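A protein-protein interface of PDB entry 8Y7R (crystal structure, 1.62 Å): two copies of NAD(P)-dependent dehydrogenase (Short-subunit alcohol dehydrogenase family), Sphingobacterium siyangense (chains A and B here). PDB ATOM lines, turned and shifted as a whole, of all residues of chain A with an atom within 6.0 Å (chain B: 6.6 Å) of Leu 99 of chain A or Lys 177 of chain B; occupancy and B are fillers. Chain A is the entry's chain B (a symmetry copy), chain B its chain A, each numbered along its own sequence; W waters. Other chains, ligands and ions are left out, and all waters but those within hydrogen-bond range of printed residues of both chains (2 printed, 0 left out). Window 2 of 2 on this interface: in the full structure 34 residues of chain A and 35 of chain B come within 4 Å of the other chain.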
ATOM      1  N   ALA A  97     -10.323  19.322 -11.976  1.00  0.00           N
ATOM      2  CA  ALA A  97     -10.323  18.557 -13.220  1.00  0.00           C
ATOM      3  C   ALA A  97     -11.363  19.116 -14.182  1.00  0.00           C
ATOM      4  O   ALA A  97     -12.574  18.955 -13.966  1.00  0.00           O
ATOM      5  CB  ALA A  97     -10.596  17.096 -12.962  1.00  0.00           C
ATOM      6  N   ALA A  98     -10.906  19.686 -15.319  1.00  0.00           N
ATOM      7  CA  ALA A  98     -11.760  20.384 -16.246  1.00  0.00           C
ATOM      8  C   ALA A  98     -10.974  20.583 -17.533  1.00  0.00           C
ATOM      9  O   ALA A  98      -9.757  20.723 -17.438  1.00  0.00           O
ATOM     10  CB  ALA A  98     -12.201  21.722 -15.676  1.00  0.00           C
ATOM     11  N   LEU A  99     -11.661  20.508 -18.680  1.00  0.00           N
ATOM     12  CA  LEU A  99     -11.069  20.861 -19.962  1.00  0.00           C
ATOM     13  C   LEU A  99     -10.638  22.322 -19.895  1.00  0.00           C
ATOM     14  O   LEU A  99     -11.215  23.121 -19.151  1.00  0.00           O
ATOM     15  CB  LEU A  99     -12.060  20.653 -21.093  1.00  0.00           C
ATOM     16  CG  LEU A  99     -12.414  19.199 -21.432  1.00  0.00           C
ATOM     17  CD1 LEU A  99     -13.603  19.125 -22.385  1.00  0.00           C
ATOM     18  CD2 LEU A  99     -11.218  18.427 -21.988  1.00  0.00           C
ATOM     19  N   THR A 100      -9.587  22.671 -20.648  1.00  0.00           N
ATOM     20  CA  THR A 100      -9.062  24.037 -20.610  1.00  0.00           C
ATOM     21  C   THR A 100     -10.198  25.081 -20.728  1.00  0.00           C
ATOM     22  O   THR A 100     -10.242  26.043 -19.964  1.00  0.00           O
ATOM     23  CB  THR A 100      -8.003  24.253 -21.703  1.00  0.00           C
ATOM     24  OG1 THR A 100      -7.015  23.244 -21.495  1.00  0.00           O
ATOM     25  CG2 THR A 100      -7.348  25.616 -21.561  1.00  0.00           C
ATOM     26  N   GLY A 101     -11.098  24.910 -21.702  1.00  0.00           N
ATOM     27  CA  GLY A 101     -12.140  25.894 -21.968  1.00  0.00           C
ATOM     28  C   GLY A 101     -13.127  26.006 -20.802  1.00  0.00           C
ATOM     29  O   GLY A 101     -13.750  27.035 -20.659  1.00  0.00           O
ATOM     30  N   ASP A 102     -13.225  24.968 -19.976  1.00  0.00           N
ATOM     31  CA  ASP A 102     -14.152  24.914 -18.860  1.00  0.00           C
ATOM     32  C   ASP A 102     -13.465  25.256 -17.547  1.00  0.00           C
ATOM     33  O   ASP A 102     -14.112  25.250 -16.509  1.00  0.00           O
ATOM     34  CB  ASP A 102     -14.789  23.540 -18.763  1.00  0.00           C
ATOM     35  CG  ASP A 102     -15.510  23.042 -20.020  1.00  0.00           C
ATOM     36  OD1 ASP A 102     -16.040  23.861 -20.768  1.00  0.00           O
ATOM     37  OD2 ASP A 102     -15.584  21.828 -20.201  1.00  0.00           O
ATOM     38  N   TYR A 103     -12.138  25.485 -17.557  1.00  0.00           N
ATOM     39  CA  TYR A 103     -11.410  25.668 -16.316  1.00  0.00           C
ATOM     40  C   TYR A 103     -11.820  26.987 -15.649  1.00  0.00           C
ATOM     41  O   TYR A 103     -11.864  28.047 -16.291  1.00  0.00           O
ATOM     42  CB  TYR A 103      -9.899  25.682 -16.590  1.00  0.00           C
ATOM     43  CG  TYR A 103      -9.110  24.971 -15.517  1.00  0.00           C
ATOM     44  CD1 TYR A 103      -8.691  25.621 -14.369  1.00  0.00           C
ATOM     45  CD2 TYR A 103      -8.762  23.611 -15.653  1.00  0.00           C
ATOM     46  CE1 TYR A 103      -8.022  24.953 -13.356  1.00  0.00           C
ATOM     47  CE2 TYR A 103      -8.007  22.969 -14.689  1.00  0.00           C
ATOM     48  CZ  TYR A 103      -7.658  23.629 -13.518  1.00  0.00           C
ATOM     49  OH  TYR A 103      -7.000  22.938 -12.523  1.00  0.00           O
ATOM     50  N   MET A 152      -7.240  17.472 -18.687  1.00  0.00           N
ATOM     51  CA  MET A 152      -8.113  17.917 -17.584  1.00  0.00           C
ATOM     52  C   MET A 152      -7.340  18.669 -16.502  1.00  0.00           C
ATOM     53  O   MET A 152      -7.915  19.225 -15.550  1.00  0.00           O
ATOM     54  CB  MET A 152      -8.924  16.783 -16.929  1.00  0.00           C
ATOM     55  CG  MET A 152      -9.708  15.944 -17.895  1.00  0.00           C
ATOM     56  SD  MET A 152     -11.006  16.907 -18.662  1.00  0.00           S
ATOM     57  CE  MET A 152     -12.124  16.762 -17.260  1.00  0.00           C
ATOM     58  N   SER A 154      -4.781  21.386 -17.200  1.00  0.00           N
ATOM     59  CA  SER A 154      -3.963  22.356 -17.919  1.00  0.00           C
ATOM     60  C   SER A 154      -3.174  23.274 -16.989  1.00  0.00           C
ATOM     61  O   SER A 154      -2.036  23.665 -17.261  1.00  0.00           O
ATOM     62  CB  SER A 154      -4.771  23.105 -18.944  1.00  0.00           C
ATOM     63  OG  SER A 154      -5.881  23.660 -18.256  1.00  0.00           O
ATOM     64  N   PHE B 120      -3.755  31.943 -21.308  1.00  0.00           N
ATOM     65  CA  PHE B 120      -4.812  31.049 -20.861  1.00  0.00           C
ATOM     66  C   PHE B 120      -6.177  31.760 -20.999  1.00  0.00           C
ATOM     67  O   PHE B 120      -7.105  31.194 -21.568  1.00  0.00           O
ATOM     68  CB  PHE B 120      -4.646  30.519 -19.449  1.00  0.00           C
ATOM     69  CG  PHE B 120      -5.936  29.974 -18.846  1.00  0.00           C
ATOM     70  CD1 PHE B 120      -6.515  28.811 -19.326  1.00  0.00           C
ATOM     71  CD2 PHE B 120      -6.604  30.715 -17.888  1.00  0.00           C
ATOM     72  CE1 PHE B 120      -7.724  28.369 -18.834  1.00  0.00           C
ATOM     73  CE2 PHE B 120      -7.804  30.256 -17.389  1.00  0.00           C
ATOM     74  CZ  PHE B 120      -8.338  29.082 -17.818  1.00  0.00           C
ATOM     75  N   LYS B 124      -9.099  30.253 -23.297  1.00  0.00           N
ATOM     76  CA  LYS B 124     -10.359  29.819 -22.701  1.00  0.00           C
ATOM     77  C   LYS B 124     -11.527  30.344 -23.535  1.00  0.00           C
ATOM     78  O   LYS B 124     -12.425  29.555 -23.908  1.00  0.00           O
ATOM     79  CB  LYS B 124     -10.441  30.297 -21.270  1.00  0.00           C
ATOM     80  CG  LYS B 124     -11.779  30.007 -20.578  1.00  0.00           C
ATOM     81  CD  LYS B 124     -11.829  30.519 -19.158  1.00  0.00           C
ATOM     82  CE  LYS B 124     -13.217  30.357 -18.558  1.00  0.00           C
ATOM     83  NZ  LYS B 124     -13.542  28.949 -18.377  1.00  0.00           N
ATOM     84  N   MET B 130     -14.821  28.751 -30.668  1.00  0.00           N
ATOM     85  CA  MET B 130     -14.494  27.772 -31.666  1.00  0.00           C
ATOM     86  C   MET B 130     -15.380  26.530 -31.508  1.00  0.00           C
ATOM     87  O   MET B 130     -15.824  26.008 -32.519  1.00  0.00           O
ATOM     88  CB  MET B 130     -12.988  27.449 -31.566  1.00  0.00           C
ATOM     89  CG  MET B 130     -12.163  28.599 -32.035  1.00  0.00           C
ATOM     90  SD  MET B 130     -10.400  28.243 -31.705  1.00  0.00           S
ATOM     91  CE  MET B 130      -9.664  29.706 -32.435  1.00  0.00           C
ATOM     92  N   GLU B 131     -15.654  26.093 -30.292  1.00  0.00           N
ATOM     93  CA  GLU B 131     -16.492  24.900 -30.120  1.00  0.00           C
ATOM     94  C   GLU B 131     -17.890  25.210 -30.693  1.00  0.00           C
ATOM     95  O   GLU B 131     -18.462  24.387 -31.386  1.00  0.00           O
ATOM     96  CB  GLU B 131     -16.644  24.524 -28.672  1.00  0.00           C
ATOM     97  CG  GLU B 131     -15.385  23.872 -28.088  1.00  0.00           C
ATOM     98  CD  GLU B 131     -15.637  23.037 -26.842  1.00  0.00           C
ATOM     99  OE1 GLU B 131     -15.766  23.648 -25.774  1.00  0.00           O
ATOM    100  OE2 GLU B 131     -15.695  21.785 -26.953  1.00  0.00           O
ATOM    101  N   GLY B 134     -17.731  24.953 -34.730  1.00  0.00           N
ATOM    102  CA  GLY B 134     -17.299  23.742 -35.377  1.00  0.00           C
ATOM    103  C   GLY B 134     -15.809  23.412 -35.225  1.00  0.00           C
ATOM    104  O   GLY B 134     -15.350  22.438 -35.832  1.00  0.00           O
ATOM    105  N   GLY B 135     -15.105  24.277 -34.519  1.00  0.00           N
ATOM    106  CA  GLY B 135     -13.679  24.102 -34.258  1.00  0.00           C
ATOM    107  C   GLY B 135     -12.863  25.324 -34.671  1.00  0.00           C
ATOM    108  O   GLY B 135     -13.366  26.395 -34.980  1.00  0.00           O
ATOM    109  N   GLY B 136     -11.542  25.144 -34.677  1.00  0.00           N
ATOM    110  CA  GLY B 136     -10.670  26.292 -34.928  1.00  0.00           C
ATOM    111  C   GLY B 136      -9.212  25.895 -34.651  1.00  0.00           C
ATOM    112  O   GLY B 136      -8.908  24.721 -34.436  1.00  0.00           O
ATOM    113  N   GLU B 173      -6.298  17.686 -25.349  1.00  0.00           N
ATOM    114  CA  GLU B 173      -7.690  17.655 -24.910  1.00  0.00           C
ATOM    115  C   GLU B 173      -8.678  17.791 -26.051  1.00  0.00           C
ATOM    116  O   GLU B 173      -9.765  17.161 -26.013  1.00  0.00           O
ATOM    117  CB  GLU B 173      -7.894  18.792 -23.914  1.00  0.00           C
ATOM    118  CG  GLU B 173      -7.343  18.556 -22.520  1.00  0.00           C
ATOM    119  CD  GLU B 173      -7.468  19.801 -21.640  1.00  0.00           C
ATOM    120  OE1 GLU B 173      -7.953  20.865 -22.108  1.00  0.00           O
ATOM    121  OE2 GLU B 173      -7.076  19.698 -20.458  1.00  0.00           O
ATOM    122  N   TYR B 174      -8.364  18.600 -27.076  1.00  0.00           N
ATOM    123  CA  TYR B 174      -9.346  18.971 -28.088  1.00  0.00           C
ATOM    124  C   TYR B 174      -9.094  18.284 -29.417  1.00  0.00           C
ATOM    125  O   TYR B 174      -9.653  18.684 -30.456  1.00  0.00           O
ATOM    126  CB  TYR B 174      -9.440  20.490 -28.205  1.00  0.00           C
ATOM    127  CG  TYR B 174     -10.081  21.166 -27.019  1.00  0.00           C
ATOM    128  CD1 TYR B 174      -9.327  21.509 -25.894  1.00  0.00           C
ATOM    129  CD2 TYR B 174     -11.476  21.326 -26.933  1.00  0.00           C
ATOM    130  CE1 TYR B 174      -9.910  22.050 -24.783  1.00  0.00           C
ATOM    131  CE2 TYR B 174     -12.056  21.887 -25.811  1.00  0.00           C
ATOM    132  CZ  TYR B 174     -11.283  22.281 -24.753  1.00  0.00           C
ATOM    133  OH  TYR B 174     -11.800  22.847 -23.622  1.00  0.00           O
ATOM    134  N   GLY B 175      -8.276  17.246 -29.373  1.00  0.00           N
ATOM    135  CA  GLY B 175      -7.869  16.571 -30.594  1.00  0.00           C
ATOM    136  C   GLY B 175      -9.063  16.072 -31.406  1.00  0.00           C
ATOM    137  O   GLY B 175      -9.031  16.143 -32.643  1.00  0.00           O
ATOM    138  N   GLN B 176     -10.069  15.547 -30.711  1.00  0.00           N
ATOM    139  CA  GLN B 176     -11.239  14.998 -31.400  1.00  0.00           C
ATOM    140  C   GLN B 176     -12.387  16.000 -31.441  1.00  0.00           C
ATOM    141  O   GLN B 176     -13.465  15.601 -31.837  1.00  0.00           O
ATOM    142  CB  GLN B 176     -11.745  13.680 -30.778  1.00  0.00           C
ATOM    143  CG  GLN B 176     -10.697  12.583 -30.935  1.00  0.00           C
ATOM    144  CD  GLN B 176     -11.084  11.201 -30.431  1.00  0.00           C
ATOM    145  OE1 GLN B 176     -10.718  10.773 -29.338  1.00  0.00           O
ATOM    146  NE2 GLN B 176     -11.740  10.463 -31.289  1.00  0.00           N
ATOM    147  N   LYS B 177     -12.149  17.275 -31.066  1.00  0.00           N
ATOM    148  CA  LYS B 177     -13.141  18.344 -31.071  1.00  0.00           C
ATOM    149  C   LYS B 177     -12.768  19.420 -32.121  1.00  0.00           C
ATOM    150  O   LYS B 177     -13.303  20.502 -32.180  1.00  0.00           O
ATOM    151  CB  LYS B 177     -13.198  18.888 -29.641  1.00  0.00           C
ATOM    152  CG  LYS B 177     -13.839  17.994 -28.593  1.00  0.00           C
ATOM    153  CD  LYS B 177     -13.465  18.423 -27.186  1.00  0.00           C
ATOM    154  CE  LYS B 177     -13.914  17.517 -26.074  1.00  0.00           C
ATOM    155  NZ  LYS B 177     -15.301  17.834 -25.725  1.00  0.00           N
ATOM    156  N   ASN B 178     -11.842  19.107 -33.025  1.00  0.00           N
ATOM    157  CA  ASN B 178     -11.508  19.916 -34.192  1.00  0.00           C
ATOM    158  C   ASN B 178     -10.931  21.278 -33.766  1.00  0.00           C
ATOM    159  O   ASN B 178     -11.132  22.267 -34.472  1.00  0.00           O
ATOM    160  CB  ASN B 178     -12.665  20.124 -35.168  1.00  0.00           C
ATOM    161  CG  ASN B 178     -12.181  20.665 -36.507  1.00  0.00           C
ATOM    162  OD1 ASN B 178     -11.064  20.350 -36.973  1.00  0.00           O
ATOM    163  ND2 ASN B 178     -12.980  21.476 -37.189  1.00  0.00           N
ATOM    164  N   ILE B 179     -10.266  21.313 -32.608  1.00  0.00           N
ATOM    165  CA  ILE B 179      -9.472  22.485 -32.262  1.00  0.00           C
ATOM    166  C   ILE B 179      -7.998  22.042 -32.213  1.00  0.00           C
ATOM    167  O   ILE B 179      -7.697  21.174 -31.408  1.00  0.00           O
ATOM    168  CB  ILE B 179      -9.910  23.143 -30.954  1.00  0.00           C
ATOM    169  CG1 ILE B 179     -11.369  23.674 -31.051  1.00  0.00           C
ATOM    170  CG2 ILE B 179      -8.968  24.286 -30.575  1.00  0.00           C
ATOM    171  CD1 ILE B 179     -11.911  24.159 -29.734  1.00  0.00           C
ATOM    172  N   ARG B 180      -7.159  22.653 -33.058  1.00  0.00           N
ATOM    173  CA  ARG B 180      -5.722  22.399 -33.000  1.00  0.00           C
ATOM    174  C   ARG B 180      -5.071  23.554 -32.256  1.00  0.00           C
ATOM    175  O   ARG B 180      -5.589  24.686 -32.268  1.00  0.00           O
ATOM    176  CB  ARG B 180      -5.126  22.245 -34.401  1.00  0.00           C
ATOM    177  CG  ARG B 180      -5.572  20.988 -35.130  1.00  0.00           C
ATOM    178  CD  ARG B 180      -4.944  20.810 -36.503  1.00  0.00           C
ATOM    179  NE  ARG B 180      -5.257  21.921 -37.396  1.00  0.00           N
ATOM    180  CZ  ARG B 180      -4.430  22.923 -37.658  1.00  0.00           C
ATOM    181  NH1 ARG B 180      -3.229  22.959 -37.096  1.00  0.00           N
ATOM    182  NH2 ARG B 180      -4.800  23.893 -38.484  1.00  0.00           N
HETATM  183  O   HOH W   1     -14.383  23.159 -23.493  1.00  0.00           O
HETATM  184  O   HOH W   2      -7.349  21.456 -18.391  1.00  0.00           O
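NZ of Lys 124 of chain B lies within hydrogen-bond range of O of Gly 101 of chain A (3.0 Å).
O of Tyr 103 of chain A is in hydrogen-bond range of NZ of Lys 124 of chain B.
The side-chain carboxylate (OE1) of Glu 173 of chain B is in hydrogen-bond range of the side-chain hydroxyl (OG1) of Thr 100 of chain A, at 2.6 Å.
The side-chain carboxylate (OE2) of Glu 173 of chain B sits at hydrogen-bond distance from the backbone NH (N) of Met 152 of chain A (2.8 Å).
The side-chain hydroxyl (OH) of Tyr 174 of chain B is in hydrogen-bond range of the backbone NH (N) of Gly 101 of chain A (2.9 Å).
No position is printed for both chains.
Of the 12 pairs that touch across the chains among the printed residues, none has its exchanged pair printed and touching as well.
The backbone NH (N) of Ile 179 of chain B is in hydrogen-bond range of the backbone carbonyl oxygen (O) of Tyr 174 of chain B (3.5 Å).
The backbone NH (N) of Ala 98 of chain A lies within hydrogen-bond range of the backbone carbonyl oxygen (O) of Met 152 of chain A (3.0 Å).
SD of Met 152 of chain A is in hydrogen-bond range of N of Leu 99 of chain A (3.7 Å).
The side-chain hydroxyl (OG1) of Thr 100 of chain A lies close to the side-chain hydroxyl (OG) of Ser 154 of chain A, at 3.5 Å.
C of Leu 99 of chain A touches OE1 of Glu 173 of chain B (3.8 Å).
Tyr 174 of chain B touches Leu 99 of chain A (OH to CB, 3.4 Å).
Leu 99 of chain A touches Lys 177 of chain B.
O of Thr 100 of chain A touches CE1 of Phe 120 of chain B, at 3.6 Å.
Thr 100 of chain A touches Tyr 174 of chain B.
NZ of Lys 124 of chain B touches C of Asp 102 of chain A, 3.8 Å away.
Tyr 103 of chain A touches Phe 120 of chain B (CB to CZ, 3.9 Å).
Hydrophobic or aromatic side chains of chain B that line the printed part of chain A: Phe 120 and Tyr 174.
Hydrophobic or aromatic side chains of chain A within 4 Å of the printed part of chain B: Leu 99 and Tyr 103.
Among the printed residues, 12 pairs touch across the chains.
Of chain B, only Glu 173, Tyr 174 and Lys 177 come within 4 Å of Leu 99 of chain A.
Printed residues of chain A within 4 Å of Phe 120 of chain B: Thr 100 (3.6 Å) and Tyr 103 (3.9 Å).
Of the printed residues of chain A, Lys 124 of chain B touches Gly 101, Asp 102 and Tyr 103.
Printed residues of chain B within 4 Å of Asp 102 of chain A: Lys 124 (3.8 Å).
Printed residues of chain B within 4 Å of Thr 100 of chain A: Phe 120 (3.6 Å), Glu 173 (2.6 Å) and Tyr 174 (3.7 Å).
Gly 134 of chain B touches none of the printed residues of chain A.
The nearest residue of chain B that does not touch Leu 99 of chain A is Glu 131 of chain B (5.7 Å).
The nearest printed residue of chain A that does not touch Lys 177 of chain B is Asp 102 of chain A (6.8 Å).
Water W1 lies within hydrogen-bond range of the side-chain hydroxyl (OH) of Tyr 174 of chain B (2.6 Å), the side-chain carboxylate (OE1) of Glu 131 of chain B (2.7 Å) and the side-chain carboxylate (OD1) of Asp 102 of chain A (3.3 Å).
Water W2 lies within hydrogen-bond range of the side-chain hydroxyl of Ser 154 of chain A (2.7 Å), the backbone carbonyl oxygen of Ala 98 of chain A (2.7 Å), the side-chain carboxylate of Glu 173 of chain B (2.7 Å) and the backbone NH of Thr 100 of chain A (3.4 Å).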
